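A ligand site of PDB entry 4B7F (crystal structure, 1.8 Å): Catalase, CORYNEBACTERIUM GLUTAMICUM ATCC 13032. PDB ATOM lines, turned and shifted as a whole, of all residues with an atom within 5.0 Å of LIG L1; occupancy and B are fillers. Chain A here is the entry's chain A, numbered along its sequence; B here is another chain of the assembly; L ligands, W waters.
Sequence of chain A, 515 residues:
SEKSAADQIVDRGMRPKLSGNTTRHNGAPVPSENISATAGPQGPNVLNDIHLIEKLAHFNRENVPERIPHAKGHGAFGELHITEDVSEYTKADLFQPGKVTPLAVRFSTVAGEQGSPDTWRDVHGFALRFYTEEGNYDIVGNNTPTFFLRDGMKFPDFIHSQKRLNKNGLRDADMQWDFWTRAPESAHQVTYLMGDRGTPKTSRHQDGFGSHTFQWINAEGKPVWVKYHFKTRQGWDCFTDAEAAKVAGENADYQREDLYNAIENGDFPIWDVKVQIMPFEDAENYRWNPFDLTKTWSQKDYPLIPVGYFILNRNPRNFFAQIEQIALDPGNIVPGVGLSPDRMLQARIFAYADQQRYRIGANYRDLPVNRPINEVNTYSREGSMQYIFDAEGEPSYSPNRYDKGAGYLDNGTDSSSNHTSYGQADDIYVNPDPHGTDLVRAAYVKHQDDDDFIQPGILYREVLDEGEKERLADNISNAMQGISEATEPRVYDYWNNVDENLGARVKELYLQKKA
A ring nitrogen (NE2) of His 70 lies close to an oxygen (O1) of LG2 L2, at 3.4 Å. O1 of LIG L1 is in hydrogen-bond range of NE2 of Gln 356 (2.9 Å). The guanidinium group of Arg 359 lies within salt-bridge range of an oxygen (O1) of LIG L1 (2.7 Å). The guanidinium group of Arg 67 lies within salt-bridge range of an oxygen (O3) of LIG L1. The guanidinium group (NH1) of Arg 106 is in salt-bridge range of an oxygen (O4) of LIG L1, at 2.7 Å. O2 of LIG L1 lies within hydrogen-bond range of NE2 of Gln 355. An iron atom (FE1) of LIG L1 is bound by the side-chain hydroxyl (OH) of Tyr 352 (2.0 Å).
An iron atom (FE1) of LIG L1 is bound by a nitrogen (N1) of LG2 L2 (1.5 Å).
O of Asn 142 is in hydrogen-bond range of N of Phe 209, 2.8 Å away. The guanidinium group of Arg 348 is in hydrogen-bond range of the backbone carbonyl oxygen of Val 140 (2.9 Å). N of Arg 106 lies within hydrogen-bond range of O of Ala 127. The backbone carbonyl oxygen (O) of Ile 326 lies within hydrogen-bond range of the guanidinium group (NH2) of Arg 67, 2.8 Å away. The side-chain hydroxyl (OG) of Ser 108 sits at hydrogen-bond distance from a ring nitrogen (ND1) of His 70, 2.8 Å away. The backbone carbonyl oxygen (O) of Ala 351 sits close to the side-chain amide oxygen (OD1) of Asn 60 of chain B (2.9 Å). O of Ile 68 lies close to OE1 of Gln 355 (2.8 Å). O of Leu 56 of chain B lies close to OD1 of Asn 60 of chain B, 3.5 Å away.
A ring nitrogen (NE2) of His 70 sits close to a nitrogen (N4) of LIG L1 (3.5 Å). Merely in contact with LIG L1: Asn 142 (3.0 Å), Gly 141 (3.1 Å), Asn 60 of chain B (3.2 Å), Arg 348 (3.3 Å), Ser 211 (3.4 Å), Met 344 (3.5 Å), Phe 155 (3.5 Å), Gly 125 (3.5 Å), His 212 (3.6 Å), Gly 210 (3.6 Å), Val 140 (3.6 Å), Gly 152 (3.6 Å), Ala 351 (3.7 Å), Ala 347 (3.7 Å), Leu 293 (3.8 Å), Phe 126 (3.8 Å), Leu 328 (3.8 Å), Ile 68 (3.8 Å), Pro 69 (3.9 Å), Ala 127 (3.9 Å) and Phe 147 (3.9 Å). Hydrophobic or aromatic side chains that line LIG L1: Pro 69, His 70, Ala 127, Val 140, Phe 147, Phe 155, His 212, Leu 293, Leu 328, Met 344, Ala 347, Ala 351 and Tyr 352. The nearest printed residue that does not touch LIG L1 is Leu 56 of chain B (4.04 Å).
Water W4 lies within hydrogen-bond range of an oxygen (O4) of LIG L1 (2.7 Å), the side-chain hydroxyl of Ser 108 (2.8 Å) and the backbone carbonyl oxygen of Arg 106 (2.8 Å). Water W3 bridges the side-chain amide nitrogen of Asn 142 and a ring nitrogen (NE2) of His 70. Water W2 bridges the side-chain hydroxyl of Ser 211 (3.0 Å) and the side-chain amide nitrogen of Asn 142 (3.1 Å).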
ATOM      1  N   ARG A  67       2.942  37.260  15.524  1.00  0.00           N
ATOM      2  CA  ARG A  67       3.014  36.306  16.634  1.00  0.00           C
ATOM      3  C   ARG A  67       4.353  35.597  16.687  1.00  0.00           C
ATOM      4  O   ARG A  67       4.884  35.188  15.657  1.00  0.00           O
ATOM      5  CB  ARG A  67       1.966  35.202  16.463  1.00  0.00           C
ATOM      6  CG  ARG A  67       0.517  35.643  16.594  1.00  0.00           C
ATOM      7  CD  ARG A  67      -0.387  34.623  15.917  1.00  0.00           C
ATOM      8  NE  ARG A  67      -1.787  34.901  16.191  1.00  0.00           N
ATOM      9  CZ  ARG A  67      -2.480  35.865  15.620  1.00  0.00           C
ATOM     10  NH1 ARG A  67      -1.906  36.669  14.714  1.00  0.00           N
ATOM     11  NH2 ARG A  67      -3.757  36.042  15.934  1.00  0.00           N
ATOM     12  N   ILE A  68       4.882  35.400  17.902  1.00  0.00           N
ATOM     13  CA  ILE A  68       5.932  34.412  18.097  1.00  0.00           C
ATOM     14  C   ILE A  68       5.469  33.363  19.113  1.00  0.00           C
ATOM     15  O   ILE A  68       5.114  33.700  20.243  1.00  0.00           O
ATOM     16  CB  ILE A  68       7.274  35.057  18.561  1.00  0.00           C
ATOM     17  CG1 ILE A  68       8.316  33.966  18.831  1.00  0.00           C
ATOM     18  CG2 ILE A  68       7.070  35.967  19.797  1.00  0.00           C
ATOM     19  CD1 ILE A  68       9.726  34.512  19.102  1.00  0.00           C
ATOM     20  N   PRO A  69       5.387  32.086  18.700  1.00  0.00           N
ATOM     21  CA  PRO A  69       5.487  31.561  17.343  1.00  0.00           C
ATOM     22  C   PRO A  69       4.094  31.600  16.702  1.00  0.00           C
ATOM     23  O   PRO A  69       3.218  32.300  17.215  1.00  0.00           O
ATOM     24  CB  PRO A  69       5.953  30.108  17.575  1.00  0.00           C
ATOM     25  CG  PRO A  69       5.521  29.769  19.004  1.00  0.00           C
ATOM     26  CD  PRO A  69       5.022  31.036  19.665  1.00  0.00           C
ATOM     27  N   HIS A  70       3.913  30.850  15.612  1.00  0.00           N
ATOM     28  CA  HIS A  70       2.619  30.724  14.907  1.00  0.00           C
ATOM     29  C   HIS A  70       2.245  31.969  14.098  1.00  0.00           C
ATOM     30  O   HIS A  70       1.060  32.255  13.895  1.00  0.00           O
ATOM     31  CB  HIS A  70       1.468  30.340  15.843  1.00  0.00           C
ATOM     32  CG  HIS A  70       1.566  28.970  16.449  1.00  0.00           C
ATOM     33  ND1 HIS A  70       0.866  27.880  15.971  1.00  0.00           N
ATOM     34  CD2 HIS A  70       2.251  28.525  17.536  1.00  0.00           C
ATOM     35  CE1 HIS A  70       1.132  26.825  16.720  1.00  0.00           C
ATOM     36  NE2 HIS A  70       1.972  27.188  17.676  1.00  0.00           N
ATOM     37  N   ARG A 106      -8.413  29.787  14.158  1.00  0.00           N
ATOM     38  CA  ARG A 106      -7.240  30.161  13.394  1.00  0.00           C
ATOM     39  C   ARG A 106      -6.365  28.928  13.259  1.00  0.00           C
ATOM     40  O   ARG A 106      -6.127  28.220  14.250  1.00  0.00           O
ATOM     41  CB  ARG A 106      -6.461  31.296  14.065  1.00  0.00           C
ATOM     42  CG  ARG A 106      -5.298  31.851  13.213  1.00  0.00           C
ATOM     43  CD  ARG A 106      -4.687  33.115  13.841  1.00  0.00           C
ATOM     44  NE  ARG A 106      -3.513  33.592  13.097  1.00  0.00           N
ATOM     45  CZ  ARG A 106      -2.272  33.122  13.260  1.00  0.00           C
ATOM     46  NH1 ARG A 106      -2.029  32.151  14.136  1.00  0.00           N
ATOM     47  NH2 ARG A 106      -1.278  33.633  12.538  1.00  0.00           N
ATOM     48  N   SER A 108      -2.511  27.531  11.658  1.00  0.00           N
ATOM     49  CA  SER A 108      -1.203  28.145  11.473  1.00  0.00           C
ATOM     50  C   SER A 108      -0.125  27.097  11.378  1.00  0.00           C
ATOM     51  O   SER A 108      -0.378  25.927  11.653  1.00  0.00           O
ATOM     52  CB  SER A 108      -0.874  29.035  12.672  1.00  0.00           C
ATOM     53  OG  SER A 108      -0.980  28.306  13.891  1.00  0.00           O
ATOM     54  N   GLY A 125      -1.141  24.732  14.151  1.00  0.00           N
ATOM     55  CA  GLY A 125      -2.019  25.208  15.206  1.00  0.00           C
ATOM     56  C   GLY A 125      -3.476  24.991  14.837  1.00  0.00           C
ATOM     57  O   GLY A 125      -3.851  25.059  13.661  1.00  0.00           O
ATOM     58  N   PHE A 126      -4.312  24.781  15.857  1.00  0.00           N
ATOM     59  CA  PHE A 126      -5.725  24.454  15.661  1.00  0.00           C
ATOM     60  C   PHE A 126      -6.427  25.160  16.809  1.00  0.00           C
ATOM     61  O   PHE A 126      -6.717  24.554  17.847  1.00  0.00           O
ATOM     62  CB  PHE A 126      -5.903  22.939  15.784  1.00  0.00           C
ATOM     63  CG  PHE A 126      -7.155  22.407  15.122  1.00  0.00           C
ATOM     64  CD1 PHE A 126      -8.407  22.708  15.634  1.00  0.00           C
ATOM     65  CD2 PHE A 126      -7.070  21.596  14.003  1.00  0.00           C
ATOM     66  CE1 PHE A 126      -9.565  22.208  15.044  1.00  0.00           C
ATOM     67  CE2 PHE A 126      -8.214  21.085  13.396  1.00  0.00           C
ATOM     68  CZ  PHE A 126      -9.471  21.397  13.920  1.00  0.00           C
ATOM     69  N   ALA A 127      -6.671  26.460  16.640  1.00  0.00           N
ATOM     70  CA  ALA A 127      -7.035  27.300  17.765  1.00  0.00           C
ATOM     71  C   ALA A 127      -8.449  27.836  17.637  1.00  0.00           C
ATOM     72  O   ALA A 127      -8.747  28.632  16.745  1.00  0.00           O
ATOM     73  CB  ALA A 127      -6.048  28.447  17.904  1.00  0.00           C
ATOM     74  N   VAL A 140      -7.055  26.406  22.550  1.00  0.00           N
ATOM     75  CA  VAL A 140      -5.964  26.764  21.672  1.00  0.00           C
ATOM     76  C   VAL A 140      -5.138  25.505  21.509  1.00  0.00           C
ATOM     77  O   VAL A 140      -4.225  25.239  22.293  1.00  0.00           O
ATOM     78  CB  VAL A 140      -5.120  27.904  22.273  1.00  0.00           C
ATOM     79  CG1 VAL A 140      -3.997  28.317  21.326  1.00  0.00           C
ATOM     80  CG2 VAL A 140      -6.018  29.123  22.559  1.00  0.00           C
ATOM     81  N   GLY A 141      -5.473  24.716  20.492  1.00  0.00           N
ATOM     82  CA  GLY A 141      -4.885  23.398  20.348  1.00  0.00           C
ATOM     83  C   GLY A 141      -3.941  23.294  19.176  1.00  0.00           C
ATOM     84  O   GLY A 141      -3.567  24.316  18.596  1.00  0.00           O
ATOM     85  N   ASN A 142      -3.545  22.067  18.836  1.00  0.00           N
ATOM     86  CA  ASN A 142      -2.638  21.825  17.701  1.00  0.00           C
ATOM     87  C   ASN A 142      -3.153  20.585  16.975  1.00  0.00           C
ATOM     88  O   ASN A 142      -4.106  19.947  17.432  1.00  0.00           O
ATOM     89  CB  ASN A 142      -1.202  21.541  18.193  1.00  0.00           C
ATOM     90  CG  ASN A 142      -0.336  22.804  18.335  1.00  0.00           C
ATOM     91  OD1 ASN A 142      -0.487  23.784  17.592  1.00  0.00           O
ATOM     92  ND2 ASN A 142       0.615  22.768  19.274  1.00  0.00           N
ATOM     93  N   PHE A 147       3.146  17.119  22.582  1.00  0.00           N
ATOM     94  CA  PHE A 147       4.058  18.221  22.233  1.00  0.00           C
ATOM     95  C   PHE A 147       5.491  17.888  22.653  1.00  0.00           C
ATOM     96  O   PHE A 147       5.737  16.827  23.255  1.00  0.00           O
ATOM     97  CB  PHE A 147       3.583  19.544  22.852  1.00  0.00           C
ATOM     98  CG  PHE A 147       4.101  20.789  22.133  1.00  0.00           C
ATOM     99  CD1 PHE A 147       3.688  21.073  20.835  1.00  0.00           C
ATOM    100  CD2 PHE A 147       4.980  21.653  22.764  1.00  0.00           C
ATOM    101  CE1 PHE A 147       4.153  22.221  20.168  1.00  0.00           C
ATOM    102  CE2 PHE A 147       5.464  22.792  22.112  1.00  0.00           C
ATOM    103  CZ  PHE A 147       5.037  23.075  20.809  1.00  0.00           C
ATOM    104  N   GLY A 152       7.476  24.657  30.787  1.00  0.00           N
ATOM    105  CA  GLY A 152       7.488  25.907  30.048  1.00  0.00           C
ATOM    106  C   GLY A 152       8.818  26.623  30.055  1.00  0.00           C
ATOM    107  O   GLY A 152       9.100  27.469  29.194  1.00  0.00           O
ATOM    108  N   PHE A 155      10.467  26.249  26.733  1.00  0.00           N
ATOM    109  CA  PHE A 155       9.747  26.608  25.517  1.00  0.00           C
ATOM    110  C   PHE A 155      10.496  27.612  24.618  1.00  0.00           C
ATOM    111  O   PHE A 155      10.599  27.386  23.413  1.00  0.00           O
ATOM    112  CB  PHE A 155       8.297  27.048  25.819  1.00  0.00           C
ATOM    113  CG  PHE A 155       7.541  27.518  24.618  1.00  0.00           C
ATOM    114  CD1 PHE A 155       6.977  26.610  23.726  1.00  0.00           C
ATOM    115  CD2 PHE A 155       7.374  28.884  24.377  1.00  0.00           C
ATOM    116  CE1 PHE A 155       6.274  27.031  22.606  1.00  0.00           C
ATOM    117  CE2 PHE A 155       6.670  29.324  23.255  1.00  0.00           C
ATOM    118  CZ  PHE A 155       6.103  28.388  22.380  1.00  0.00           C
ATOM    119  N   PHE A 209      -6.487  18.830  18.448  1.00  0.00           N
ATOM    120  CA  PHE A 209      -6.460  18.294  19.810  1.00  0.00           C
ATOM    121  C   PHE A 209      -6.199  19.418  20.787  1.00  0.00           C
ATOM    122  O   PHE A 209      -5.509  20.390  20.446  1.00  0.00           O
ATOM    123  CB  PHE A 209      -5.324  17.276  19.976  1.00  0.00           C
ATOM    124  CG  PHE A 209      -5.327  16.179  18.953  1.00  0.00           C
ATOM    125  CD1 PHE A 209      -4.728  16.365  17.718  1.00  0.00           C
ATOM    126  CD2 PHE A 209      -5.922  14.945  19.244  1.00  0.00           C
ATOM    127  CE1 PHE A 209      -4.716  15.356  16.766  1.00  0.00           C
ATOM    128  CE2 PHE A 209      -5.918  13.927  18.298  1.00  0.00           C
ATOM    129  CZ  PHE A 209      -5.315  14.131  17.047  1.00  0.00           C
ATOM    130  N   GLY A 210      -6.706  19.275  22.002  1.00  0.00           N
ATOM    131  CA  GLY A 210      -6.387  20.228  23.050  1.00  0.00           C
ATOM    132  C   GLY A 210      -5.002  19.917  23.594  1.00  0.00           C
ATOM    133  O   GLY A 210      -4.364  20.771  24.239  1.00  0.00           O
ATOM    134  N   SER A 211      -4.555  18.691  23.329  1.00  0.00           N
ATOM    135  CA  SER A 211      -3.248  18.171  23.749  1.00  0.00           C
ATOM    136  C   SER A 211      -3.139  17.987  25.261  1.00  0.00           C
ATOM    137  O   SER A 211      -2.964  16.850  25.751  1.00  0.00           O
ATOM    138  CB  SER A 211      -2.087  19.020  23.190  1.00  0.00           C
ATOM    139  OG  SER A 211      -2.197  19.175  21.785  1.00  0.00           O
ATOM    140  N   HIS A 212      -3.208  19.083  26.016  1.00  0.00           N
ATOM    141  CA  HIS A 212      -3.150  19.011  27.472  1.00  0.00           C
ATOM    142  C   HIS A 212      -4.329  18.278  28.081  1.00  0.00           C
ATOM    143  O   HIS A 212      -5.426  18.237  27.513  1.00  0.00           O
ATOM    144  CB  HIS A 212      -3.163  20.409  28.112  1.00  0.00           C
ATOM    145  CG  HIS A 212      -2.126  21.356  27.593  1.00  0.00           C
ATOM    146  ND1 HIS A 212      -0.795  21.274  27.942  1.00  0.00           N
ATOM    147  CD2 HIS A 212      -2.247  22.431  26.776  1.00  0.00           C
ATOM    148  CE1 HIS A 212      -0.133  22.257  27.353  1.00  0.00           C
ATOM    149  NE2 HIS A 212      -0.984  22.967  26.636  1.00  0.00           N
ATOM    150  N   LEU A 293       2.550  16.377  29.204  1.00  0.00           N
ATOM    151  CA  LEU A 293       2.108  16.674  27.851  1.00  0.00           C
ATOM    152  C   LEU A 293       2.719  15.754  26.813  1.00  0.00           C
ATOM    153  O   LEU A 293       2.110  15.482  25.758  1.00  0.00           O
ATOM    154  CB  LEU A 293       2.459  18.125  27.522  1.00  0.00           C
ATOM    155  CG  LEU A 293       2.131  18.676  26.144  1.00  0.00           C
ATOM    156  CD1 LEU A 293       0.641  18.512  25.819  1.00  0.00           C
ATOM    157  CD2 LEU A 293       2.545  20.148  26.086  1.00  0.00           C
ATOM    158  N   ILE A 326      -6.969  38.614  16.124  1.00  0.00           N
ATOM    159  CA  ILE A 326      -7.597  37.744  17.101  1.00  0.00           C
ATOM    160  C   ILE A 326      -6.558  37.404  18.171  1.00  0.00           C
ATOM    161  O   ILE A 326      -5.355  37.297  17.886  1.00  0.00           O
ATOM    162  CB  ILE A 326      -8.251  36.451  16.500  1.00  0.00           C
ATOM    163  CG1 ILE A 326      -9.277  35.874  17.464  1.00  0.00           C
ATOM    164  CG2 ILE A 326      -7.203  35.386  16.173  1.00  0.00           C
ATOM    165  CD1 ILE A 326     -10.189  34.836  16.816  1.00  0.00           C
ATOM    166  N   ALA A 327      -7.018  37.295  19.413  1.00  0.00           N
ATOM    167  CA  ALA A 327      -6.139  37.055  20.542  1.00  0.00           C
ATOM    168  C   ALA A 327      -6.594  35.792  21.253  1.00  0.00           C
ATOM    169  O   ALA A 327      -7.311  35.837  22.257  1.00  0.00           O
ATOM    170  CB  ALA A 327      -6.124  38.256  21.500  1.00  0.00           C
ATOM    171  N   LEU A 328      -6.170  34.654  20.705  1.00  0.00           N
ATOM    172  CA  LEU A 328      -6.591  33.352  21.221  1.00  0.00           C
ATOM    173  C   LEU A 328      -5.710  32.976  22.401  1.00  0.00           C
ATOM    174  O   LEU A 328      -4.498  33.179  22.366  1.00  0.00           O
ATOM    175  CB  LEU A 328      -6.532  32.317  20.100  1.00  0.00           C
ATOM    176  CG  LEU A 328      -7.555  32.594  18.996  1.00  0.00           C
ATOM    177  CD1 LEU A 328      -7.153  31.929  17.704  1.00  0.00           C
ATOM    178  CD2 LEU A 328      -8.935  32.095  19.431  1.00  0.00           C
ATOM    179  N   MET A 344       3.455  22.897  31.200  1.00  0.00           N
ATOM    180  CA  MET A 344       3.408  23.623  29.925  1.00  0.00           C
ATOM    181  C   MET A 344       2.131  24.436  29.882  1.00  0.00           C
ATOM    182  O   MET A 344       2.158  25.631  29.563  1.00  0.00           O
ATOM    183  CB  MET A 344       3.441  22.642  28.753  1.00  0.00           C
ATOM    184  CG  MET A 344       4.790  21.933  28.608  1.00  0.00           C
ATOM    185  SD  MET A 344       6.056  22.930  27.793  1.00  0.00           S
ATOM    186  CE  MET A 344       5.495  22.821  26.090  1.00  0.00           C
ATOM    187  N   ALA A 347       2.316  27.495  32.210  1.00  0.00           N
ATOM    188  CA  ALA A 347       3.109  28.564  31.610  1.00  0.00           C
ATOM    189  C   ALA A 347       2.299  29.307  30.538  1.00  0.00           C
ATOM    190  O   ALA A 347       2.373  30.538  30.439  1.00  0.00           O
ATOM    191  CB  ALA A 347       4.393  28.004  31.013  1.00  0.00           C
ATOM    192  N   ARG A 348       1.546  28.562  29.734  1.00  0.00           N
ATOM    193  CA  ARG A 348       0.765  29.155  28.656  1.00  0.00           C
ATOM    194  C   ARG A 348      -0.300  30.112  29.210  1.00  0.00           C
ATOM    195  O   ARG A 348      -0.607  31.130  28.600  1.00  0.00           O
ATOM    196  CB  ARG A 348       0.071  28.066  27.821  1.00  0.00           C
ATOM    197  CG  ARG A 348       1.009  27.152  27.066  1.00  0.00           C
ATOM    198  CD  ARG A 348       0.234  26.096  26.292  1.00  0.00           C
ATOM    199  NE  ARG A 348      -0.445  26.674  25.128  1.00  0.00           N
ATOM    200  CZ  ARG A 348      -1.572  26.213  24.596  1.00  0.00           C
ATOM    201  NH1 ARG A 348      -2.187  25.167  25.146  1.00  0.00           N
ATOM    202  NH2 ARG A 348      -2.115  26.809  23.541  1.00  0.00           N
ATOM    203  N   ALA A 351       1.383  33.267  29.369  1.00  0.00           N
ATOM    204  CA  ALA A 351       2.145  33.772  28.223  1.00  0.00           C
ATOM    205  C   ALA A 351       1.345  34.473  27.129  1.00  0.00           C
ATOM    206  O   ALA A 351       1.833  35.436  26.509  1.00  0.00           O
ATOM    207  CB  ALA A 351       2.979  32.648  27.618  1.00  0.00           C
ATOM    208  N   TYR A 352       0.148  33.974  26.832  1.00  0.00           N
ATOM    209  CA  TYR A 352      -0.558  34.447  25.639  1.00  0.00           C
ATOM    210  C   TYR A 352      -1.042  35.875  25.828  1.00  0.00           C
ATOM    211  O   TYR A 352      -0.765  36.745  25.001  1.00  0.00           O
ATOM    212  CB  TYR A 352      -1.707  33.507  25.249  1.00  0.00           C
ATOM    213  CG  TYR A 352      -1.239  32.178  24.681  1.00  0.00           C
ATOM    214  CD1 TYR A 352      -0.492  31.287  25.441  1.00  0.00           C
ATOM    215  CD2 TYR A 352      -1.588  31.801  23.391  1.00  0.00           C
ATOM    216  CE1 TYR A 352      -0.081  30.063  24.934  1.00  0.00           C
ATOM    217  CE2 TYR A 352      -1.173  30.576  22.870  1.00  0.00           C
ATOM    218  CZ  TYR A 352      -0.418  29.717  23.645  1.00  0.00           C
ATOM    219  OH  TYR A 352      -0.012  28.502  23.128  1.00  0.00           O
ATOM    220  N   GLN A 355       1.749  38.333  25.682  1.00  0.00           N
ATOM    221  CA  GLN A 355       2.217  38.703  24.344  1.00  0.00           C
ATOM    222  C   GLN A 355       1.185  39.599  23.663  1.00  0.00           C
ATOM    223  O   GLN A 355       1.532  40.555  22.947  1.00  0.00           O
ATOM    224  CB  GLN A 355       2.508  37.482  23.455  1.00  0.00           C
ATOM    225  CG  GLN A 355       3.026  37.941  22.080  1.00  0.00           C
ATOM    226  CD  GLN A 355       3.670  36.853  21.239  1.00  0.00           C
ATOM    227  OE1 GLN A 355       4.172  35.843  21.747  1.00  0.00           O
ATOM    228  NE2 GLN A 355       3.667  37.074  19.929  1.00  0.00           N
ATOM    229  N   GLN A 356      -0.092  39.303  23.880  1.00  0.00           N
ATOM    230  CA  GLN A 356      -1.154  40.050  23.234  1.00  0.00           C
ATOM    231  C   GLN A 356      -1.213  41.507  23.698  1.00  0.00           C
ATOM    232  O   GLN A 356      -1.451  42.416  22.896  1.00  0.00           O
ATOM    233  CB  GLN A 356      -2.492  39.315  23.428  1.00  0.00           C
ATOM    234  CG  GLN A 356      -2.547  38.044  22.591  1.00  0.00           C
ATOM    235  CD  GLN A 356      -3.405  36.933  23.197  1.00  0.00           C
ATOM    236  OE1 GLN A 356      -4.047  37.126  24.233  1.00  0.00           O
ATOM    237  NE2 GLN A 356      -3.407  35.765  22.545  1.00  0.00           N
ATOM    238  N   ARG A 359       1.734  42.858  21.447  1.00  0.00           N
ATOM    239  CA  ARG A 359       1.655  42.789  19.998  1.00  0.00           C
ATOM    240  C   ARG A 359       0.401  43.487  19.437  1.00  0.00           C
ATOM    241  O   ARG A 359       0.423  44.022  18.321  1.00  0.00           O
ATOM    242  CB  ARG A 359       1.790  41.335  19.529  1.00  0.00           C
ATOM    243  CG  ARG A 359       0.614  40.767  18.776  1.00  0.00           C
ATOM    244  CD  ARG A 359       0.845  39.295  18.383  1.00  0.00           C
ATOM    245  NE  ARG A 359      -0.289  38.483  18.799  1.00  0.00           N
ATOM    246  CZ  ARG A 359      -1.475  38.516  18.210  1.00  0.00           C
ATOM    247  NH1 ARG A 359      -1.678  39.331  17.175  1.00  0.00           N
ATOM    248  NH2 ARG A 359      -2.471  37.733  18.651  1.00  0.00           N
ATOM    249  N   LEU B  56       9.997  34.090  29.613  1.00  0.00           N
ATOM    250  CA  LEU B  56       8.804  34.063  28.751  1.00  0.00           C
ATOM    251  C   LEU B  56       8.394  35.451  28.260  1.00  0.00           C
ATOM    252  O   LEU B  56       8.002  35.621  27.113  1.00  0.00           O
ATOM    253  CB  LEU B  56       7.625  33.414  29.487  1.00  0.00           C
ATOM    254  CG  LEU B  56       7.714  31.923  29.819  1.00  0.00           C
ATOM    255  CD1 LEU B  56       6.509  31.510  30.695  1.00  0.00           C
ATOM    256  CD2 LEU B  56       7.789  31.075  28.551  1.00  0.00           C
ATOM    257  N   ASN B  60       8.237  36.859  24.488  1.00  0.00           N
ATOM    258  CA  ASN B  60       6.986  37.389  23.958  1.00  0.00           C
ATOM    259  C   ASN B  60       7.134  38.718  23.240  1.00  0.00           C
ATOM    260  O   ASN B  60       6.223  39.152  22.522  1.00  0.00           O
ATOM    261  CB  ASN B  60       5.961  37.577  25.104  1.00  0.00           C
ATOM    262  CG  ASN B  60       5.228  36.294  25.475  1.00  0.00           C
ATOM    263  OD1 ASN B  60       4.612  36.211  26.546  1.00  0.00           O
ATOM    264  ND2 ASN B  60       5.271  35.316  24.604  1.00  0.00           N
HETATM  265  C1  LIG L   1       0.759  30.810  19.842  1.00  0.00           C
HETATM  266  C2  LIG L   1       3.095  30.458  24.075  1.00  0.00           C
HETATM  267  C3  LIG L   1       2.924  25.613  23.759  1.00  0.00           C
HETATM  268  C4  LIG L   1      -0.628  26.158  20.521  1.00  0.00           C
HETATM  269  C5  LIG L   1       1.412  31.136  21.003  1.00  0.00           C
HETATM  270  C6  LIG L   1       1.699  32.480  21.483  1.00  0.00           C
HETATM  271  C7  LIG L   1       2.340  32.364  22.651  1.00  0.00           C
HETATM  272  C8  LIG L   1       2.483  30.963  22.954  1.00  0.00           C
HETATM  273  C9  LIG L   1       2.831  33.520  23.548  1.00  0.00           C
HETATM  274  C10 LIG L   1       1.336  33.807  20.781  1.00  0.00           C
HETATM  275  C11 LIG L   1      -0.136  34.126  21.088  1.00  0.00           C
HETATM  276  C12 LIG L   1      -0.541  35.466  20.521  1.00  0.00           C
HETATM  277  O1  LIG L   1      -1.754  35.613  20.158  1.00  0.00           O
HETATM  278  O2  LIG L   1       0.331  36.381  20.422  1.00  0.00           O
HETATM  279  C13 LIG L   1       3.270  29.124  24.330  1.00  0.00           C
HETATM  280  C14 LIG L   1       3.991  28.605  25.465  1.00  0.00           C
HETATM  281  C15 LIG L   1       3.963  27.255  25.374  1.00  0.00           C
HETATM  282  C16 LIG L   1       3.203  26.902  24.204  1.00  0.00           C
HETATM  283  C17 LIG L   1       4.667  29.496  26.528  1.00  0.00           C
HETATM  284  C18 LIG L   1       4.569  26.209  26.342  1.00  0.00           C
HETATM  285  C19 LIG L   1       4.872  26.501  27.611  1.00  0.00           C
HETATM  286  C20 LIG L   1       1.819  25.348  22.985  1.00  0.00           C
HETATM  287  C21 LIG L   1       1.003  24.152  22.978  1.00  0.00           C
HETATM  288  C22 LIG L   1       0.024  24.312  22.071  1.00  0.00           C
HETATM  289  C23 LIG L   1       0.180  25.626  21.498  1.00  0.00           C
HETATM  290  C24 LIG L   1       1.298  22.901  23.852  1.00  0.00           C
HETATM  291  C25 LIG L   1      -1.143  23.379  21.668  1.00  0.00           C
HETATM  292  C26 LIG L   1      -1.687  22.456  22.482  1.00  0.00           C
HETATM  293  C27 LIG L   1      -0.536  27.415  20.001  1.00  0.00           C
HETATM  294  C28 LIG L   1      -1.339  27.894  18.903  1.00  0.00           C
HETATM  295  C29 LIG L   1      -0.918  29.330  18.687  1.00  0.00           C
HETATM  296  C30 LIG L   1       0.097  29.604  19.677  1.00  0.00           C
HETATM  297  C31 LIG L   1      -2.399  27.097  18.119  1.00  0.00           C
HETATM  298  C32 LIG L   1      -1.486  30.289  17.642  1.00  0.00           C
HETATM  299  C33 LIG L   1      -2.845  30.764  18.141  1.00  0.00           C
HETATM  300  C34 LIG L   1      -3.394  31.562  17.005  1.00  0.00           C
HETATM  301  O3  LIG L   1      -3.513  32.822  17.162  1.00  0.00           O
HETATM  302  O4  LIG L   1      -3.692  30.941  15.948  1.00  0.00           O
HETATM  303  N1  LIG L   1       1.909  30.222  21.932  1.00  0.00           N
HETATM  304  N2  LIG L   1       2.800  28.065  23.579  1.00  0.00           N
HETATM  305  N3  LIG L   1       1.275  26.242  22.072  1.00  0.00           N
HETATM  306  N4  LIG L   1       0.296  28.446  20.430  1.00  0.00           N
HETATM  307 FE1  LIG L   1       1.626  28.210  21.970  1.00  0.00          FE
HETATM  308  N1  LG2 L   2       2.766  27.941  21.047  1.00  0.00           N
HETATM  309  O1  LG2 L   2       3.623  27.303  20.650  1.00  0.00           O
HETATM  310  O   HOH W   1      -3.954  34.595  18.942  1.00  0.00           O
HETATM  311  O   HOH W   2       0.462  20.326  21.153  1.00  0.00           O
HETATM  312  O   HOH W   3       2.599  24.866  19.404  1.00  0.00           O
HETATM  313  O   HOH W   4      -3.480  28.457  15.040  1.00  0.00           O
